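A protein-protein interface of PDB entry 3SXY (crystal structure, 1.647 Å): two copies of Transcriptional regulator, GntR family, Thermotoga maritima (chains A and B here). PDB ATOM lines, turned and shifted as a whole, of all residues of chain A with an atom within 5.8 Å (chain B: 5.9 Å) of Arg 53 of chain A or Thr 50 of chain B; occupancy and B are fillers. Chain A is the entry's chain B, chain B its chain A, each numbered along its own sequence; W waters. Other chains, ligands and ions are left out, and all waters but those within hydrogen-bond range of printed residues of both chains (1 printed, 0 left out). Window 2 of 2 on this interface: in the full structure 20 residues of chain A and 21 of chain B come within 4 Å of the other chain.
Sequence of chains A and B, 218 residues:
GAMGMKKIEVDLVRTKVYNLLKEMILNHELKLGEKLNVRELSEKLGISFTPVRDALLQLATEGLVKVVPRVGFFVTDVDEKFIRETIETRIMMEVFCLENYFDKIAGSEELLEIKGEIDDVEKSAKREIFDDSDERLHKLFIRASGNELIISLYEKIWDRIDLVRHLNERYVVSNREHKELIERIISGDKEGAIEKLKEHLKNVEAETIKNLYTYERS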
ATOM      1  N   VAL A  38      -9.824  20.954  -1.980  1.00  0.00           N
ATOM      2  CA  VAL A  38      -9.213  20.666  -3.254  1.00  0.00           C
ATOM      3  C   VAL A  38      -9.905  19.525  -3.937  1.00  0.00           C
ATOM      4  O   VAL A  38     -10.132  19.566  -5.087  1.00  0.00           O
ATOM      5  CB  VAL A  38      -7.725  20.372  -3.136  1.00  0.00           C
ATOM      6  CG1 VAL A  38      -7.172  19.821  -4.401  1.00  0.00           C
ATOM      7  CG2 VAL A  38      -7.015  21.597  -2.803  1.00  0.00           C
ATOM      8  N   PHE A  49      -6.302  17.061  -9.387  1.00  0.00           N
ATOM      9  CA  PHE A  49      -5.958  17.821  -8.179  1.00  0.00           C
ATOM     10  C   PHE A  49      -4.777  18.775  -8.314  1.00  0.00           C
ATOM     11  O   PHE A  49      -4.743  19.793  -7.712  1.00  0.00           O
ATOM     12  CB  PHE A  49      -5.588  16.910  -7.013  1.00  0.00           C
ATOM     13  CG  PHE A  49      -6.562  15.831  -6.728  1.00  0.00           C
ATOM     14  CD1 PHE A  49      -7.895  16.097  -6.657  1.00  0.00           C
ATOM     15  CD2 PHE A  49      -6.142  14.569  -6.497  1.00  0.00           C
ATOM     16  CE1 PHE A  49      -8.801  15.109  -6.401  1.00  0.00           C
ATOM     17  CE2 PHE A  49      -7.037  13.576  -6.232  1.00  0.00           C
ATOM     18  CZ  PHE A  49      -8.364  13.851  -6.188  1.00  0.00           C
ATOM     19  N   THR A  50      -3.797  18.365  -9.083  1.00  0.00           N
ATOM     20  CA  THR A  50      -2.547  19.131  -9.206  1.00  0.00           C
ATOM     21  C   THR A  50      -2.773  20.569  -9.641  1.00  0.00           C
ATOM     22  O   THR A  50      -2.267  21.474  -8.986  1.00  0.00           O
ATOM     23  CB  THR A  50      -1.541  18.396 -10.139  1.00  0.00           C
ATOM     24  OG1 THR A  50      -1.178  17.144  -9.523  1.00  0.00           O
ATOM     25  CG2 THR A  50      -0.296  19.211 -10.342  1.00  0.00           C
ATOM     26  N   PRO A  51      -3.508  20.780 -10.741  1.00  0.00           N
ATOM     27  CA  PRO A  51      -3.645  22.174 -11.161  1.00  0.00           C
ATOM     28  C   PRO A  51      -4.553  22.985 -10.236  1.00  0.00           C
ATOM     29  O   PRO A  51      -4.420  24.224 -10.171  1.00  0.00           O
ATOM     30  CB  PRO A  51      -4.286  22.047 -12.535  1.00  0.00           C
ATOM     31  CG  PRO A  51      -5.052  20.739 -12.477  1.00  0.00           C
ATOM     32  CD  PRO A  51      -4.007  19.888 -11.803  1.00  0.00           C
ATOM     33  N   VAL A  52      -5.488  22.324  -9.557  1.00  0.00           N
ATOM     34  CA  VAL A  52      -6.273  23.029  -8.542  1.00  0.00           C
ATOM     35  C   VAL A  52      -5.393  23.540  -7.397  1.00  0.00           C
ATOM     36  O   VAL A  52      -5.488  24.708  -7.002  1.00  0.00           O
ATOM     37  CB  VAL A  52      -7.425  22.170  -8.036  1.00  0.00           C
ATOM     38  CG1 VAL A  52      -8.111  22.872  -6.890  1.00  0.00           C
ATOM     39  CG2 VAL A  52      -8.396  21.908  -9.185  1.00  0.00           C
ATOM     40  N   ARG A  53      -4.562  22.665  -6.849  1.00  0.00           N
ATOM     41  CA  ARG A  53      -3.631  23.039  -5.824  1.00  0.00           C
ATOM     42  C   ARG A  53      -2.687  24.143  -6.333  1.00  0.00           C
ATOM     43  O   ARG A  53      -2.457  25.115  -5.598  1.00  0.00           O
ATOM     44  CB  ARG A  53      -2.876  21.811  -5.310  1.00  0.00           C
ATOM     45  CG  ARG A  53      -1.789  22.166  -4.293  1.00  0.00           C
ATOM     46  CD  ARG A  53      -1.097  20.960  -3.746  1.00  0.00           C
ATOM     47  NE  ARG A  53      -0.048  21.382  -2.835  1.00  0.00           N
ATOM     48  CZ  ARG A  53       1.187  21.672  -3.208  1.00  0.00           C
ATOM     49  NH1 ARG A  53       1.539  21.532  -4.483  1.00  0.00           N
ATOM     50  NH2 ARG A  53       2.042  22.025  -2.275  1.00  0.00           N
ATOM     51  N   ASP A  54      -2.128  24.006  -7.543  1.00  0.00           N
ATOM     52  CA  ASP A  54      -1.227  25.010  -8.122  1.00  0.00           C
ATOM     53  C   ASP A  54      -1.933  26.395  -8.136  1.00  0.00           C
ATOM     54  O   ASP A  54      -1.342  27.422  -7.731  1.00  0.00           O
ATOM     55  CB  ASP A  54      -0.854  24.677  -9.591  1.00  0.00           C
ATOM     56  CG  ASP A  54       0.005  23.405  -9.769  1.00  0.00           C
ATOM     57  OD1 ASP A  54       0.649  22.937  -8.782  1.00  0.00           O
ATOM     58  OD2 ASP A  54       0.028  22.902 -10.959  1.00  0.00           O
ATOM     59  N   ALA A  55      -3.180  26.413  -8.576  1.00  0.00           N
ATOM     60  CA  ALA A  55      -3.976  27.630  -8.700  1.00  0.00           C
ATOM     61  C   ALA A  55      -4.251  28.263  -7.328  1.00  0.00           C
ATOM     62  O   ALA A  55      -4.162  29.473  -7.151  1.00  0.00           O
ATOM     63  CB  ALA A  55      -5.273  27.361  -9.421  1.00  0.00           C
ATOM     64  N   LEU A  56      -4.583  27.453  -6.331  1.00  0.00           N
ATOM     65  CA  LEU A  56      -4.843  27.966  -5.004  1.00  0.00           C
ATOM     66  C   LEU A  56      -3.606  28.566  -4.428  1.00  0.00           C
ATOM     67  O   LEU A  56      -3.698  29.550  -3.732  1.00  0.00           O
ATOM     68  CB  LEU A  56      -5.459  26.940  -4.049  1.00  0.00           C
ATOM     69  CG  LEU A  56      -6.824  26.466  -4.522  1.00  0.00           C
ATOM     70  CD1 LEU A  56      -7.292  25.365  -3.548  1.00  0.00           C
ATOM     71  CD2 LEU A  56      -7.845  27.549  -4.602  1.00  0.00           C
ATOM     72  N   LEU A  57      -2.455  27.959  -4.675  1.00  0.00           N
ATOM     73  CA  LEU A  57      -1.210  28.539  -4.171  1.00  0.00           C
ATOM     74  C   LEU A  57      -0.909  29.859  -4.861  1.00  0.00           C
ATOM     75  O   LEU A  57      -0.411  30.809  -4.210  1.00  0.00           O
ATOM     76  CB  LEU A  57      -0.072  27.567  -4.400  1.00  0.00           C
ATOM     77  CG  LEU A  57      -0.068  26.372  -3.476  1.00  0.00           C
ATOM     78  CD1 LEU A  57       0.971  25.340  -3.890  1.00  0.00           C
ATOM     79  CD2 LEU A  57       0.190  26.776  -2.054  1.00  0.00           C
ATOM     80  N   GLN A  58      -1.204  29.988  -6.123  1.00  0.00           N
ATOM     81  CA  GLN A  58      -0.970  31.264  -6.761  1.00  0.00           C
ATOM     82  C   GLN A  58      -1.939  32.331  -6.232  1.00  0.00           C
ATOM     83  O   GLN A  58      -1.565  33.489  -5.950  1.00  0.00           O
ATOM     84  CB  GLN A  58      -1.127  31.140  -8.223  1.00  0.00           C
ATOM     85  CG  GLN A  58      -0.940  32.501  -8.889  1.00  0.00           C
ATOM     86  CD  GLN A  58      -0.978  32.443 -10.415  1.00  0.00           C
ATOM     87  OE1 GLN A  58      -0.874  31.381 -11.020  1.00  0.00           O
ATOM     88  NE2 GLN A  58      -1.138  33.586 -11.021  1.00  0.00           N
ATOM     89  N   PHE A  73      -6.893  25.704   2.883  1.00  0.00           N
ATOM     90  CA  PHE A  73      -7.106  26.911   2.104  1.00  0.00           C
ATOM     91  C   PHE A  73      -8.453  27.533   2.352  1.00  0.00           C
ATOM     92  O   PHE A  73      -9.420  26.874   2.469  1.00  0.00           O
ATOM     93  CB  PHE A  73      -7.055  26.650   0.618  1.00  0.00           C
ATOM     94  CG  PHE A  73      -5.782  26.106   0.123  1.00  0.00           C
ATOM     95  CD1 PHE A  73      -4.754  26.925  -0.202  1.00  0.00           C
ATOM     96  CD2 PHE A  73      -5.653  24.793  -0.129  1.00  0.00           C
ATOM     97  CE1 PHE A  73      -3.594  26.435  -0.722  1.00  0.00           C
ATOM     98  CE2 PHE A  73      -4.486  24.288  -0.647  1.00  0.00           C
ATOM     99  CZ  PHE A  73      -3.462  25.117  -0.943  1.00  0.00           C
ATOM    100  N   ARG B  14       8.377  24.465   1.071  1.00  0.00           N
ATOM    101  CA  ARG B  14       7.892  25.325  -0.001  1.00  0.00           C
ATOM    102  C   ARG B  14       8.468  26.730   0.131  1.00  0.00           C
ATOM    103  O   ARG B  14       8.853  27.349  -0.862  1.00  0.00           O
ATOM    104  CB  ARG B  14       6.363  25.384   0.016  1.00  0.00           C
ATOM    105  CG  ARG B  14       5.692  24.387  -0.915  1.00  0.00           C
ATOM    106  CD  ARG B  14       4.305  24.857  -1.320  1.00  0.00           C
ATOM    107  NE  ARG B  14       3.661  25.637  -0.266  1.00  0.00           N
ATOM    108  CZ  ARG B  14       2.643  25.200   0.468  1.00  0.00           C
ATOM    109  NH1 ARG B  14       2.148  23.987   0.266  1.00  0.00           N
ATOM    110  NH2 ARG B  14       2.120  25.979   1.406  1.00  0.00           N
ATOM    111  N   VAL B  38      13.546  20.465 -12.646  1.00  0.00           N
ATOM    112  CA  VAL B  38      13.100  20.224 -11.296  1.00  0.00           C
ATOM    113  C   VAL B  38      13.853  19.095 -10.573  1.00  0.00           C
ATOM    114  O   VAL B  38      14.231  19.229  -9.449  1.00  0.00           O
ATOM    115  CB  VAL B  38      11.611  19.912 -11.233  1.00  0.00           C
ATOM    116  CG1 VAL B  38      11.211  19.673  -9.867  1.00  0.00           C
ATOM    117  CG2 VAL B  38      10.804  21.047 -11.757  1.00  0.00           C
ATOM    118  N   SER B  48      12.548  17.331  -1.877  1.00  0.00           N
ATOM    119  CA  SER B  48      11.734  16.562  -2.814  1.00  0.00           C
ATOM    120  C   SER B  48      11.209  17.443  -3.964  1.00  0.00           C
ATOM    121  O   SER B  48      11.244  18.675  -3.907  1.00  0.00           O
ATOM    122  CB  SER B  48      10.590  15.873  -2.089  1.00  0.00           C
ATOM    123  OG  SER B  48       9.678  16.829  -1.627  1.00  0.00           O
ATOM    124  N   PHE B  49      10.684  16.763  -4.943  1.00  0.00           N
ATOM    125  CA  PHE B  49      10.265  17.299  -6.201  1.00  0.00           C
ATOM    126  C   PHE B  49       9.179  18.367  -6.069  1.00  0.00           C
ATOM    127  O   PHE B  49       9.300  19.411  -6.571  1.00  0.00           O
ATOM    128  CB  PHE B  49       9.772  16.144  -7.031  1.00  0.00           C
ATOM    129  CG  PHE B  49       9.350  16.503  -8.384  1.00  0.00           C
ATOM    130  CD1 PHE B  49      10.214  16.383  -9.425  1.00  0.00           C
ATOM    131  CD2 PHE B  49       8.083  16.958  -8.633  1.00  0.00           C
ATOM    132  CE1 PHE B  49       9.834  16.712 -10.685  1.00  0.00           C
ATOM    133  CE2 PHE B  49       7.698  17.284  -9.887  1.00  0.00           C
ATOM    134  CZ  PHE B  49       8.577  17.158 -10.920  1.00  0.00           C
ATOM    135  N   THR B  50       8.142  18.044  -5.346  1.00  0.00           N
ATOM    136  CA  THR B  50       6.950  18.894  -5.227  1.00  0.00           C
ATOM    137  C   THR B  50       7.259  20.306  -4.718  1.00  0.00           C
ATOM    138  O   THR B  50       6.857  21.289  -5.306  1.00  0.00           O
ATOM    139  CB  THR B  50       5.853  18.237  -4.345  1.00  0.00           C
ATOM    140  OG1 THR B  50       5.423  17.043  -4.986  1.00  0.00           O
ATOM    141  CG2 THR B  50       4.634  19.122  -4.191  1.00  0.00           C
ATOM    142  N   PRO B  51       7.989  20.450  -3.592  1.00  0.00           N
ATOM    143  CA  PRO B  51       8.210  21.850  -3.233  1.00  0.00           C
ATOM    144  C   PRO B  51       9.172  22.621  -4.116  1.00  0.00           C
ATOM    145  O   PRO B  51       9.128  23.859  -4.124  1.00  0.00           O
ATOM    146  CB  PRO B  51       8.799  21.767  -1.844  1.00  0.00           C
ATOM    147  CG  PRO B  51       9.383  20.456  -1.761  1.00  0.00           C
ATOM    148  CD  PRO B  51       8.419  19.560  -2.507  1.00  0.00           C
ATOM    149  N   VAL B  52      10.097  21.920  -4.797  1.00  0.00           N
ATOM    150  CA  VAL B  52      10.879  22.583  -5.837  1.00  0.00           C
ATOM    151  C   VAL B  52       9.961  23.132  -6.954  1.00  0.00           C
ATOM    152  O   VAL B  52      10.056  24.296  -7.327  1.00  0.00           O
ATOM    153  CB  VAL B  52      11.993  21.691  -6.388  1.00  0.00           C
ATOM    154  CG1 VAL B  52      12.711  22.361  -7.535  1.00  0.00           C
ATOM    155  CG2 VAL B  52      12.966  21.331  -5.254  1.00  0.00           C
ATOM    156  N   ARG B  53       9.082  22.274  -7.483  1.00  0.00           N
ATOM    157  CA  ARG B  53       8.164  22.684  -8.535  1.00  0.00           C
ATOM    158  C   ARG B  53       7.264  23.818  -8.045  1.00  0.00           C
ATOM    159  O   ARG B  53       7.037  24.792  -8.747  1.00  0.00           O
ATOM    160  CB  ARG B  53       7.309  21.488  -8.992  1.00  0.00           C
ATOM    161  CG  ARG B  53       6.297  21.846 -10.102  1.00  0.00           C
ATOM    162  CD  ARG B  53       5.543  20.617 -10.600  1.00  0.00           C
ATOM    163  NE  ARG B  53       4.480  20.997 -11.534  1.00  0.00           N
ATOM    164  CZ  ARG B  53       3.275  21.417 -11.178  1.00  0.00           C
ATOM    165  NH1 ARG B  53       2.966  21.523  -9.886  1.00  0.00           N
ATOM    166  NH2 ARG B  53       2.368  21.747 -12.105  1.00  0.00           N
ATOM    167  N   ASP B  54       6.756  23.685  -6.799  1.00  0.00           N
ATOM    168  CA  ASP B  54       5.906  24.745  -6.264  1.00  0.00           C
ATOM    169  C   ASP B  54       6.630  26.086  -6.261  1.00  0.00           C
ATOM    170  O   ASP B  54       6.062  27.147  -6.580  1.00  0.00           O
ATOM    171  CB  ASP B  54       5.500  24.493  -4.792  1.00  0.00           C
ATOM    172  CG  ASP B  54       4.566  23.288  -4.586  1.00  0.00           C
ATOM    173  OD1 ASP B  54       3.834  22.822  -5.500  1.00  0.00           O
ATOM    174  OD2 ASP B  54       4.532  22.752  -3.416  1.00  0.00           O
ATOM    175  N   ALA B  55       7.871  26.037  -5.815  1.00  0.00           N
ATOM    176  CA  ALA B  55       8.704  27.266  -5.736  1.00  0.00           C
ATOM    177  C   ALA B  55       9.015  27.891  -7.099  1.00  0.00           C
ATOM    178  O   ALA B  55       8.946  29.114  -7.233  1.00  0.00           O
ATOM    179  CB  ALA B  55       9.966  26.958  -5.058  1.00  0.00           C
HETATM  180  O   HOH W   1       2.303  24.335  -7.048  1.00  0.00           O
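Thr 50 of chain A touches none of the printed residues of chain B. Val 52 of chain A touches none of the printed residues of chain B. Printed residues of chain A within 4 Å of Arg 14 of chain B: Arg 53 (3.2 Å) and Leu 57 (3.9 Å). Thr 50 of chain B touches just one residue of chain A: Arg 53 (3.9 Å). Of the printed residues of chain A, Arg 53 of chain B touches Asp 54. The nearest residue of chain B that does not touch Arg 53 of chain A is Arg 53 of chain B (5.6 Å). The nearest printed residue of chain A that does not touch Thr 50 of chain B is Asp 54 of chain A (7.2 Å).
Arg 53 of chain A touches Thr 50 of chain B, but with the chains exchanged Thr 50 of chain A does not touch Arg 53 of chain B (4.02 Å). Arg 53 of chain A touches Asp 54 of chain B, and with the chains exchanged Asp 54 of chain A touches Arg 53 of chain B. 8 positions are printed for both chains. Of the 5 pairs that touch across the chains among the printed residues, 2 have their exchanged pair printed and touching as well.
Of the 10 printed residues of chain B, 4 touch a printed residue of chain A.
Among the printed residues, merely in contact across the chains: Arg 53 of chain A with Thr 50 of chain B (3.9 Å) and Leu 57 of chain A with Arg 14 of chain B (3.9 Å).
Water W1 lies within hydrogen-bond range of the side-chain carboxylate (OD1) of Asp 54 of chain B and the side-chain carboxylate (OD1) of Asp 54 of chain A.
The guanidinium group (NH2) of Arg 53 of chain B is in salt-bridge range of the side-chain carboxylate (OD2) of Asp 54 of chain A, 2.9 Å away. The side-chain carboxylate of Asp 54 of chain B lies within salt-bridge range of the guanidinium group of Arg 53 of chain A (2.8 Å). The guanidinium group (NH1) of Arg 14 of chain B lies close to the guanidinium group (NH2) of Arg 53 of chain A (3.2 Å).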
